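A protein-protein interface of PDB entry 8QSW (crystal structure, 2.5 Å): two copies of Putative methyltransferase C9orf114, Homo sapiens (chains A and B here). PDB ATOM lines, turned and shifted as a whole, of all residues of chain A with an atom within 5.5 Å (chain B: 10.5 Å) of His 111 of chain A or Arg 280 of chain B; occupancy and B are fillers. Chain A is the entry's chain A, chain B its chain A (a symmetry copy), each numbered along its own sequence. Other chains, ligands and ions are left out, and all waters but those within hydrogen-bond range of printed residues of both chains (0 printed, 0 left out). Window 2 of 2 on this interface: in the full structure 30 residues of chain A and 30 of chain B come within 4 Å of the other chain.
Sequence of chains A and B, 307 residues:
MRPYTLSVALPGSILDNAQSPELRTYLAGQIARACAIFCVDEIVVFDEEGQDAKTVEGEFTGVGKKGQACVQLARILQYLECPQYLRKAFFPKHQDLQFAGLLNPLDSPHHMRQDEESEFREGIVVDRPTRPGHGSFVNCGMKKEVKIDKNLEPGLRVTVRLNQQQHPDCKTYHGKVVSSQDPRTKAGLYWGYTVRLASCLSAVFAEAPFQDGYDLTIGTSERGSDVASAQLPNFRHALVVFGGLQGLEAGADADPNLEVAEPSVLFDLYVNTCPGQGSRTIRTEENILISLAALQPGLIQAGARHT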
ATOM      1  N   ARG A  33     -36.338  23.492 -19.924  1.00  0.00           N
ATOM      2  CA  ARG A  33     -35.359  23.378 -18.855  1.00  0.00           C
ATOM      3  C   ARG A  33     -34.794  21.969 -18.880  1.00  0.00           C
ATOM      4  O   ARG A  33     -33.571  21.798 -18.777  1.00  0.00           O
ATOM      5  CB  ARG A  33     -35.917  23.780 -17.493  1.00  0.00           C
ATOM      6  CG  ARG A  33     -36.088  25.278 -17.351  1.00  0.00           C
ATOM      7  CD  ARG A  33     -35.990  25.629 -15.873  1.00  0.00           C
ATOM      8  NE  ARG A  33     -34.722  26.270 -15.596  1.00  0.00           N
ATOM      9  CZ  ARG A  33     -33.736  25.747 -14.904  1.00  0.00           C
ATOM     10  NH1 ARG A  33     -33.935  24.680 -14.178  1.00  0.00           N
ATOM     11  NH2 ARG A  33     -32.560  26.336 -14.907  1.00  0.00           N
ATOM     12  N   LEU A  80     -37.434  30.798 -25.197  1.00  0.00           N
ATOM     13  CA  LEU A  80     -36.646  30.602 -23.988  1.00  0.00           C
ATOM     14  C   LEU A  80     -35.172  30.392 -24.301  1.00  0.00           C
ATOM     15  O   LEU A  80     -34.335  30.649 -23.439  1.00  0.00           O
ATOM     16  CB  LEU A  80     -37.165  29.371 -23.246  1.00  0.00           C
ATOM     17  CG  LEU A  80     -38.525  29.522 -22.574  1.00  0.00           C
ATOM     18  CD1 LEU A  80     -38.895  28.223 -21.900  1.00  0.00           C
ATOM     19  CD2 LEU A  80     -38.507  30.667 -21.572  1.00  0.00           C
ATOM     20  N   GLU A  81     -34.876  29.836 -25.481  1.00  0.00           N
ATOM     21  CA  GLU A  81     -33.507  29.608 -25.916  1.00  0.00           C
ATOM     22  C   GLU A  81     -32.879  30.948 -26.291  1.00  0.00           C
ATOM     23  O   GLU A  81     -31.766  31.253 -25.907  1.00  0.00           O
ATOM     24  CB  GLU A  81     -33.507  28.662 -27.123  1.00  0.00           C
ATOM     25  CG  GLU A  81     -32.116  28.241 -27.632  1.00  0.00           C
ATOM     26  CD  GLU A  81     -31.265  29.236 -28.395  1.00  0.00           C
ATOM     27  OE1 GLU A  81     -31.833  30.054 -29.138  1.00  0.00           O
ATOM     28  OE2 GLU A  81     -30.022  29.150 -28.288  1.00  0.00           O
ATOM     29  N   CYS A  82     -33.628  31.777 -27.015  1.00  0.00           N
ATOM     30  CA  CYS A  82     -33.098  33.049 -27.453  1.00  0.00           C
ATOM     31  C   CYS A  82     -32.677  33.906 -26.269  1.00  0.00           C
ATOM     32  O   CYS A  82     -33.454  34.145 -25.360  1.00  0.00           O
ATOM     33  CB  CYS A  82     -34.144  33.802 -28.240  1.00  0.00           C
ATOM     34  SG  CYS A  82     -33.512  35.403 -28.755  1.00  0.00           S
ATOM     35  N   PRO A  83     -31.429  34.406 -26.238  1.00  0.00           N
ATOM     36  CA  PRO A  83     -30.999  35.340 -25.208  1.00  0.00           C
ATOM     37  C   PRO A  83     -31.981  36.473 -25.062  1.00  0.00           C
ATOM     38  O   PRO A  83     -32.654  36.812 -26.032  1.00  0.00           O
ATOM     39  CB  PRO A  83     -29.717  35.933 -25.782  1.00  0.00           C
ATOM     40  CG  PRO A  83     -29.152  34.833 -26.651  1.00  0.00           C
ATOM     41  CD  PRO A  83     -30.361  34.120 -27.198  1.00  0.00           C
ATOM     42  N   ARG A  87     -34.816  39.136 -27.607  1.00  0.00           N
ATOM     43  CA  ARG A  87     -36.203  38.709 -27.669  1.00  0.00           C
ATOM     44  C   ARG A  87     -37.066  39.778 -28.350  1.00  0.00           C
ATOM     45  O   ARG A  87     -37.761  39.446 -29.315  1.00  0.00           O
ATOM     46  CB  ARG A  87     -36.669  38.301 -26.269  1.00  0.00           C
ATOM     47  CG  ARG A  87     -35.951  37.081 -25.713  1.00  0.00           C
ATOM     48  CD  ARG A  87     -36.701  36.431 -24.574  1.00  0.00           C
ATOM     49  NE  ARG A  87     -36.032  35.178 -24.271  1.00  0.00           N
ATOM     50  CZ  ARG A  87     -35.664  34.765 -23.062  1.00  0.00           C
ATOM     51  NH1 ARG A  87     -36.084  35.397 -21.982  1.00  0.00           N
ATOM     52  NH2 ARG A  87     -34.892  33.697 -22.927  1.00  0.00           N
ATOM     53  N   LEU A 106     -33.652  29.540 -18.609  1.00  0.00           N
ATOM     54  CA  LEU A 106     -32.699  28.455 -18.800  1.00  0.00           C
ATOM     55  C   LEU A 106     -31.345  28.755 -18.150  1.00  0.00           C
ATOM     56  O   LEU A 106     -30.627  27.824 -17.784  1.00  0.00           O
ATOM     57  CB  LEU A 106     -32.559  28.156 -20.290  1.00  0.00           C
ATOM     58  CG  LEU A 106     -33.879  27.955 -21.036  1.00  0.00           C
ATOM     59  CD1 LEU A 106     -33.631  27.425 -22.424  1.00  0.00           C
ATOM     60  CD2 LEU A 106     -34.802  27.014 -20.302  1.00  0.00           C
ATOM     61  N   ASP A 107     -30.980  30.016 -17.932  1.00  0.00           N
ATOM     62  CA  ASP A 107     -29.693  30.281 -17.294  1.00  0.00           C
ATOM     63  C   ASP A 107     -28.580  29.485 -17.992  1.00  0.00           C
ATOM     64  O   ASP A 107     -27.703  28.884 -17.352  1.00  0.00           O
ATOM     65  CB  ASP A 107     -29.750  29.952 -15.804  1.00  0.00           C
ATOM     66  CG  ASP A 107     -30.664  30.866 -15.008  1.00  0.00           C
ATOM     67  OD1 ASP A 107     -31.017  31.912 -15.567  1.00  0.00           O
ATOM     68  OD2 ASP A 107     -31.014  30.530 -13.816  1.00  0.00           O
ATOM     69  N   SER A 108     -28.620  29.490 -19.331  1.00  0.00           N
ATOM     70  CA  SER A 108     -27.644  28.764 -20.122  1.00  0.00           C
ATOM     71  C   SER A 108     -26.409  29.611 -20.396  1.00  0.00           C
ATOM     72  O   SER A 108     -26.414  30.824 -20.253  1.00  0.00           O
ATOM     73  CB  SER A 108     -28.264  28.220 -21.358  1.00  0.00           C
ATOM     74  OG  SER A 108     -28.899  26.980 -21.025  1.00  0.00           O
ATOM     75  N   PRO A 109     -25.258  29.006 -20.738  1.00  0.00           N
ATOM     76  CA  PRO A 109     -24.032  29.803 -20.823  1.00  0.00           C
ATOM     77  C   PRO A 109     -24.107  31.012 -21.760  1.00  0.00           C
ATOM     78  O   PRO A 109     -23.322  31.936 -21.597  1.00  0.00           O
ATOM     79  CB  PRO A 109     -22.980  28.758 -21.202  1.00  0.00           C
ATOM     80  CG  PRO A 109     -23.548  27.446 -20.666  1.00  0.00           C
ATOM     81  CD  PRO A 109     -25.038  27.557 -20.904  1.00  0.00           C
ATOM     82  N   HIS A 110     -25.087  31.075 -22.667  1.00  0.00           N
ATOM     83  CA  HIS A 110     -25.170  32.195 -23.590  1.00  0.00           C
ATOM     84  C   HIS A 110     -26.169  33.246 -23.130  1.00  0.00           C
ATOM     85  O   HIS A 110     -26.512  34.135 -23.898  1.00  0.00           O
ATOM     86  CB  HIS A 110     -25.482  31.724 -25.013  1.00  0.00           C
ATOM     87  CG  HIS A 110     -26.731  30.937 -25.196  1.00  0.00           C
ATOM     88  ND1 HIS A 110     -26.953  29.722 -24.582  1.00  0.00           N
ATOM     89  CD2 HIS A 110     -27.792  31.164 -25.976  1.00  0.00           C
ATOM     90  CE1 HIS A 110     -28.128  29.253 -24.973  1.00  0.00           C
ATOM     91  NE2 HIS A 110     -28.662  30.118 -25.807  1.00  0.00           N
ATOM     92  N   HIS A 111     -26.657  33.115 -21.897  1.00  0.00           N
ATOM     93  CA  HIS A 111     -27.592  34.059 -21.314  1.00  0.00           C
ATOM     94  C   HIS A 111     -26.839  34.822 -20.233  1.00  0.00           C
ATOM     95  O   HIS A 111     -26.643  34.339 -19.130  1.00  0.00           O
ATOM     96  CB  HIS A 111     -28.774  33.336 -20.668  1.00  0.00           C
ATOM     97  CG  HIS A 111     -29.664  32.591 -21.592  1.00  0.00           C
ATOM     98  ND1 HIS A 111     -29.307  32.222 -22.872  1.00  0.00           N
ATOM     99  CD2 HIS A 111     -30.916  32.124 -21.396  1.00  0.00           C
ATOM    100  CE1 HIS A 111     -30.328  31.574 -23.431  1.00  0.00           C
ATOM    101  NE2 HIS A 111     -31.305  31.499 -22.557  1.00  0.00           N
ATOM    102  N   MET A 112     -26.410  36.025 -20.546  1.00  0.00           N
ATOM    103  CA  MET A 112     -25.479  36.730 -19.689  1.00  0.00           C
ATOM    104  C   MET A 112     -26.017  38.134 -19.515  1.00  0.00           C
ATOM    105  O   MET A 112     -26.811  38.579 -20.323  1.00  0.00           O
ATOM    106  CB  MET A 112     -24.110  36.802 -20.356  1.00  0.00           C
ATOM    107  CG  MET A 112     -24.223  37.005 -21.861  1.00  0.00           C
ATOM    108  SD  MET A 112     -22.700  36.551 -22.594  1.00  0.00           S
ATOM    109  CE  MET A 112     -23.150  35.030 -23.414  1.00  0.00           C
ATOM    110  N   ARG A 113     -25.600  38.809 -18.454  1.00  0.00           N
ATOM    111  CA  ARG A 113     -25.921  40.216 -18.300  1.00  0.00           C
ATOM    112  C   ARG A 113     -25.099  41.000 -19.313  1.00  0.00           C
ATOM    113  O   ARG A 113     -24.160  40.463 -19.887  1.00  0.00           O
ATOM    114  CB  ARG A 113     -25.583  40.699 -16.890  1.00  0.00           C
ATOM    115  CG  ARG A 113     -26.204  39.881 -15.769  1.00  0.00           C
ATOM    116  CD  ARG A 113     -25.515  40.247 -14.480  1.00  0.00           C
ATOM    117  NE  ARG A 113     -25.970  39.409 -13.392  1.00  0.00           N
ATOM    118  CZ  ARG A 113     -25.859  39.733 -12.110  1.00  0.00           C
ATOM    119  NH1 ARG A 113     -25.295  40.879 -11.765  1.00  0.00           N
ATOM    120  NH2 ARG A 113     -26.324  38.918 -11.179  1.00  0.00           N
ATOM    121  N   GLU A 116     -21.268  41.198 -18.222  1.00  0.00           N
ATOM    122  CA  GLU A 116     -20.595  39.931 -17.975  1.00  0.00           C
ATOM    123  C   GLU A 116     -19.588  39.727 -19.093  1.00  0.00           C
ATOM    124  O   GLU A 116     -19.975  39.774 -20.256  1.00  0.00           O
ATOM    125  CB  GLU A 116     -21.633  38.814 -17.928  1.00  0.00           C
ATOM    126  CG  GLU A 116     -21.389  37.795 -16.830  1.00  0.00           C
ATOM    127  CD  GLU A 116     -22.551  36.836 -16.609  1.00  0.00           C
ATOM    128  OE1 GLU A 116     -23.665  37.312 -16.279  1.00  0.00           O
ATOM    129  OE2 GLU A 116     -22.348  35.611 -16.778  1.00  0.00           O
ATOM    130  N   SER B 221     -25.313  18.141  -4.485  1.00  0.00           N
ATOM    131  CA  SER B 221     -24.622  19.395  -4.707  1.00  0.00           C
ATOM    132  C   SER B 221     -23.894  19.332  -6.046  1.00  0.00           C
ATOM    133  O   SER B 221     -23.348  18.297  -6.411  1.00  0.00           O
ATOM    134  CB  SER B 221     -23.650  19.656  -3.588  1.00  0.00           C
ATOM    135  OG  SER B 221     -23.179  20.991  -3.630  1.00  0.00           O
ATOM    136  N   GLU B 222     -23.852  20.445  -6.779  1.00  0.00           N
ATOM    137  CA  GLU B 222     -22.907  20.533  -7.880  1.00  0.00           C
ATOM    138  C   GLU B 222     -21.471  20.569  -7.333  1.00  0.00           C
ATOM    139  O   GLU B 222     -20.559  20.307  -8.106  1.00  0.00           O
ATOM    140  CB  GLU B 222     -23.310  21.632  -8.885  1.00  0.00           C
ATOM    141  CG  GLU B 222     -22.932  23.061  -8.525  1.00  0.00           C
ATOM    142  CD  GLU B 222     -22.901  24.011  -9.717  1.00  0.00           C
ATOM    143  OE1 GLU B 222     -22.234  23.679 -10.735  1.00  0.00           O
ATOM    144  OE2 GLU B 222     -23.521  25.099  -9.626  1.00  0.00           O
ATOM    145  N   ARG B 223     -21.256  20.823  -6.018  1.00  0.00           N
ATOM    146  CA  ARG B 223     -19.918  20.823  -5.405  1.00  0.00           C
ATOM    147  C   ARG B 223     -19.451  19.405  -5.057  1.00  0.00           C
ATOM    148  O   ARG B 223     -18.317  19.234  -4.638  1.00  0.00           O
ATOM    149  CB  ARG B 223     -19.845  21.622  -4.090  1.00  0.00           C
ATOM    150  CG  ARG B 223     -20.158  23.112  -4.177  1.00  0.00           C
ATOM    151  CD  ARG B 223     -19.115  23.836  -4.996  1.00  0.00           C
ATOM    152  NE  ARG B 223     -19.230  25.288  -4.919  1.00  0.00           N
ATOM    153  CZ  ARG B 223     -18.259  26.108  -4.518  1.00  0.00           C
ATOM    154  NH1 ARG B 223     -17.178  25.632  -3.926  1.00  0.00           N
ATOM    155  NH2 ARG B 223     -18.385  27.412  -4.673  1.00  0.00           N
ATOM    156  N   GLY B 244     -32.190  23.988  -0.823  1.00  0.00           N
ATOM    157  CA  GLY B 244     -33.027  24.912  -1.560  1.00  0.00           C
ATOM    158  C   GLY B 244     -32.274  25.478  -2.759  1.00  0.00           C
ATOM    159  O   GLY B 244     -31.232  24.969  -3.158  1.00  0.00           O
ATOM    160  N   LEU B 245     -32.865  26.517  -3.333  1.00  0.00           N
ATOM    161  CA  LEU B 245     -32.192  27.527  -4.120  1.00  0.00           C
ATOM    162  C   LEU B 245     -30.832  27.889  -3.507  1.00  0.00           C
ATOM    163  O   LEU B 245     -29.850  28.038  -4.227  1.00  0.00           O
ATOM    164  CB  LEU B 245     -33.185  28.695  -4.155  1.00  0.00           C
ATOM    165  CG  LEU B 245     -32.655  30.068  -4.545  1.00  0.00           C
ATOM    166  CD1 LEU B 245     -32.052  30.031  -5.943  1.00  0.00           C
ATOM    167  CD2 LEU B 245     -33.773  31.102  -4.450  1.00  0.00           C
ATOM    168  N   ASN B 272     -22.676  15.140  -6.887  1.00  0.00           N
ATOM    169  CA  ASN B 272     -23.202  15.792  -8.068  1.00  0.00           C
ATOM    170  C   ASN B 272     -23.778  14.724  -9.005  1.00  0.00           C
ATOM    171  O   ASN B 272     -23.044  13.870  -9.518  1.00  0.00           O
ATOM    172  CB  ASN B 272     -22.097  16.597  -8.745  1.00  0.00           C
ATOM    173  CG  ASN B 272     -22.582  17.226 -10.027  1.00  0.00           C
ATOM    174  OD1 ASN B 272     -23.342  16.613 -10.772  1.00  0.00           O
ATOM    175  ND2 ASN B 272     -22.181  18.460 -10.267  1.00  0.00           N
ATOM    176  N   CYS B 274     -25.582  15.371 -11.834  1.00  0.00           N
ATOM    177  CA  CYS B 274     -25.746  15.782 -13.208  1.00  0.00           C
ATOM    178  C   CYS B 274     -24.487  16.479 -13.709  1.00  0.00           C
ATOM    179  O   CYS B 274     -24.372  17.701 -13.735  1.00  0.00           O
ATOM    180  CB  CYS B 274     -26.960  16.684 -13.344  1.00  0.00           C
ATOM    181  SG  CYS B 274     -27.387  16.966 -15.081  1.00  0.00           S
ATOM    182  N   GLY B 276     -21.774  18.310 -15.886  1.00  0.00           N
ATOM    183  CA  GLY B 276     -21.780  19.192 -17.040  1.00  0.00           C
ATOM    184  C   GLY B 276     -23.175  19.654 -17.455  1.00  0.00           C
ATOM    185  O   GLY B 276     -23.512  19.635 -18.638  1.00  0.00           O
ATOM    186  N   GLN B 277     -23.966  20.069 -16.465  1.00  0.00           N
ATOM    187  CA  GLN B 277     -25.260  20.662 -16.693  1.00  0.00           C
ATOM    188  C   GLN B 277     -25.181  21.902 -17.582  1.00  0.00           C
ATOM    189  O   GLN B 277     -24.198  22.635 -17.543  1.00  0.00           O
ATOM    190  CB  GLN B 277     -25.831  21.058 -15.344  1.00  0.00           C
ATOM    191  CG  GLN B 277     -25.035  22.145 -14.628  1.00  0.00           C
ATOM    192  CD  GLN B 277     -25.334  22.122 -13.143  1.00  0.00           C
ATOM    193  OE1 GLN B 277     -24.910  21.212 -12.424  1.00  0.00           O
ATOM    194  NE2 GLN B 277     -26.107  23.101 -12.691  1.00  0.00           N
ATOM    195  N   GLY B 278     -26.250  22.181 -18.342  1.00  0.00           N
ATOM    196  CA  GLY B 278     -26.212  23.314 -19.259  1.00  0.00           C
ATOM    197  C   GLY B 278     -27.052  24.497 -18.785  1.00  0.00           C
ATOM    198  O   GLY B 278     -27.227  25.478 -19.486  1.00  0.00           O
ATOM    199  N   SER B 279     -27.556  24.365 -17.582  1.00  0.00           N
ATOM    200  CA  SER B 279     -28.153  25.424 -16.796  1.00  0.00           C
ATOM    201  C   SER B 279     -27.254  25.714 -15.596  1.00  0.00           C
ATOM    202  O   SER B 279     -26.761  24.745 -14.994  1.00  0.00           O
ATOM    203  CB  SER B 279     -29.508  24.945 -16.287  1.00  0.00           C
ATOM    204  OG  SER B 279     -30.468  25.959 -16.491  1.00  0.00           O
ATOM    205  N   ARG B 280     -27.155  26.998 -15.186  1.00  0.00           N
ATOM    206  CA  ARG B 280     -26.449  27.376 -13.953  1.00  0.00           C
ATOM    207  C   ARG B 280     -27.069  26.766 -12.684  1.00  0.00           C
ATOM    208  O   ARG B 280     -26.370  26.611 -11.702  1.00  0.00           O
ATOM    209  CB  ARG B 280     -26.432  28.894 -13.742  1.00  0.00           C
ATOM    210  CG  ARG B 280     -25.378  29.634 -14.548  1.00  0.00           C
ATOM    211  CD  ARG B 280     -25.720  31.112 -14.724  1.00  0.00           C
ATOM    212  NE  ARG B 280     -25.266  31.608 -16.026  1.00  0.00           N
ATOM    213  CZ  ARG B 280     -26.031  32.128 -16.989  1.00  0.00           C
ATOM    214  NH1 ARG B 280     -27.301  32.444 -16.781  1.00  0.00           N
ATOM    215  NH2 ARG B 280     -25.490  32.368 -18.170  1.00  0.00           N
ATOM    216  N   THR B 281     -28.367  26.448 -12.707  1.00  0.00           N
ATOM    217  CA  THR B 281     -29.154  26.067 -11.539  1.00  0.00           C
ATOM    218  C   THR B 281     -30.089  24.896 -11.837  1.00  0.00           C
ATOM    219  O   THR B 281     -30.803  24.868 -12.827  1.00  0.00           O
ATOM    220  CB  THR B 281     -30.083  27.216 -11.114  1.00  0.00           C
ATOM    221  OG1 THR B 281     -30.721  27.710 -12.303  1.00  0.00           O
ATOM    222  CG2 THR B 281     -29.354  28.342 -10.406  1.00  0.00           C
ATOM    223  N   ILE B 282     -30.182  23.963 -10.916  1.00  0.00           N
ATOM    224  CA  ILE B 282     -31.230  22.976 -11.019  1.00  0.00           C
ATOM    225  C   ILE B 282     -32.174  23.200  -9.859  1.00  0.00           C
ATOM    226  O   ILE B 282     -31.763  23.170  -8.707  1.00  0.00           O
ATOM    227  CB  ILE B 282     -30.638  21.557 -11.061  1.00  0.00           C
ATOM    228  CG1 ILE B 282     -29.616  21.470 -12.203  1.00  0.00           C
ATOM    229  CG2 ILE B 282     -31.729  20.500 -11.199  1.00  0.00           C
ATOM    230  CD1 ILE B 282     -28.954  20.109 -12.325  1.00  0.00           C
ATOM    231  N   ARG B 283     -33.442  23.383 -10.208  1.00  0.00           N
ATOM    232  CA  ARG B 283     -34.514  23.456  -9.238  1.00  0.00           C
ATOM    233  C   ARG B 283     -34.757  22.096  -8.617  1.00  0.00           C
ATOM    234  O   ARG B 283     -34.470  21.058  -9.202  1.00  0.00           O
ATOM    235  CB  ARG B 283     -35.757  24.014  -9.907  1.00  0.00           C
ATOM    236  CG  ARG B 283     -35.473  25.376 -10.520  1.00  0.00           C
ATOM    237  CD  ARG B 283     -36.374  26.435  -9.907  1.00  0.00           C
ATOM    238  NE  ARG B 283     -37.707  26.116 -10.350  1.00  0.00           N
ATOM    239  CZ  ARG B 283     -37.996  26.009 -11.626  1.00  0.00           C
ATOM    240  NH1 ARG B 283     -37.177  26.548 -12.513  1.00  0.00           N
ATOM    241  NH2 ARG B 283     -39.117  25.422 -12.001  1.00  0.00           N
ATOM    242  N   GLU B 286     -36.805  19.544 -10.062  1.00  0.00           N
ATOM    243  CA  GLU B 286     -35.984  18.960 -11.106  1.00  0.00           C
ATOM    244  C   GLU B 286     -34.965  18.007 -10.499  1.00  0.00           C
ATOM    245  O   GLU B 286     -34.739  16.892 -10.972  1.00  0.00           O
ATOM    246  CB  GLU B 286     -35.303  20.064 -11.913  1.00  0.00           C
ATOM    247  CG  GLU B 286     -36.308  20.904 -12.695  1.00  0.00           C
ATOM    248  CD  GLU B 286     -35.786  22.205 -13.276  1.00  0.00           C
ATOM    249  OE1 GLU B 286     -34.681  22.603 -12.828  1.00  0.00           O
ATOM    250  OE2 GLU B 286     -36.493  22.830 -14.160  1.00  0.00           O
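The guanidinium group (NH2) of Arg 33 of chain A is in hydrogen-bond range of the side-chain hydroxyl (OG) of Ser 279 of chain B (2.7 Å). NH2 of Arg 33 of chain A is in hydrogen-bond range of O of Thr 281 of chain B. The side-chain carboxylate of Glu 286 of chain B is in salt-bridge range of the guanidinium group of Arg 33 of chain A, 2.6 Å away. OD1 of Asp 107 of chain A lies within salt-bridge range of NH1 of Arg 280 of chain B (3.9 Å). The side-chain carboxylate (OD2) of Asp 107 of chain A lies within hydrogen-bond range of the side-chain hydroxyl (OG1) of Thr 281 of chain B (3.2 Å). OG of Ser 108 of chain A is in hydrogen-bond range of O of Gly 278 of chain B (2.7 Å). O of Ser 108 of chain A sits at hydrogen-bond distance from NH2 of Arg 280 of chain B, 2.8 Å away. O of His 111 of chain A lies within hydrogen-bond range of NH2 of Arg 280 of chain B, 2.5 Å away. The backbone carbonyl oxygen (O) of Leu 106 of chain A sits close to the side-chain hydroxyl (OG) of Ser 279 of chain B (2.3 Å).
O of Leu 80 of chain A sits at hydrogen-bond distance from NE2 of His 111 of chain A, at 3.3 Å. O of Glu 81 of chain A lies close to NE2 of His 111 of chain A (3.4 Å). The backbone carbonyl oxygen of Ser 279 of chain B sits at hydrogen-bond distance from the side-chain amide nitrogen of Gln 277 of chain B, 2.9 Å away. The side-chain carboxylate (OE1) of Glu 286 of chain B is in hydrogen-bond range of the backbone NH (N) of Arg 283 of chain B.
Arg 33 of chain A touches Arg 283 of chain B. Ser 279 of chain B touches Asp 107 of chain A. Pro 109 of chain A touches Gly 278 of chain B (CD to O, 3.3 Å). NH2 of Arg 280 of chain B touches CA of Pro 109 of chain A (3.97 Å).
His 111 of chain A touches just one residue of chain B: Arg 280. Of the printed residues of chain A, Arg 280 of chain B touches Asp 107 (2.9 Å), Ser 108 (2.8 Å), Pro 109 (3.97 Å) and His 111 (2.5 Å). Of chain B, only Ser 279 (2.3 Å) comes within 4 Å of Leu 106 of chain A. Printed residues of chain B within 4 Å of Pro 109 of chain A: Gly 278 and Arg 280. No residue of chain B comes within 4 Å of His 110 of chain A. Of the printed residues of chain A, Thr 281 of chain B touches Arg 33 (3.1 Å) and Asp 107 (3.2 Å). Of the printed residues of chain A, Glu 286 of chain B touches Arg 33. Printed residues of chain B within 4 Å of Arg 33 of chain A: Ser 279, Thr 281, Arg 283 and Glu 286. Of the printed residues of chain A, Arg 283 of chain B touches Arg 33 (3.7 Å). Of the printed residues of chain A, Ser 279 of chain B touches Arg 33, Leu 106 and Asp 107. Cys 82 of chain A touches none of the printed residues of chain B. The nearest residue of chain B that does not touch His 111 of chain A is Gly 278 of chain B (7.8 Å).
Of the 15 printed residues of chain A, 6 touch a printed residue of chain B. Hydrophobic or aromatic side chains of chain A that line the printed part of chain B: Pro 109. Among the printed residues, Asp or Glu carboxylates within 4 Å of a Lys or Arg side-chain nitrogen of the other chain: Arg 33 of chain A with Glu 286 of chain B and Asp 107 of chain A with Arg 280 of chain B.
No position is printed for both chains. Of the 13 pairs that touch across the chains among the printed residues, none has its exchanged pair printed and touching as well.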
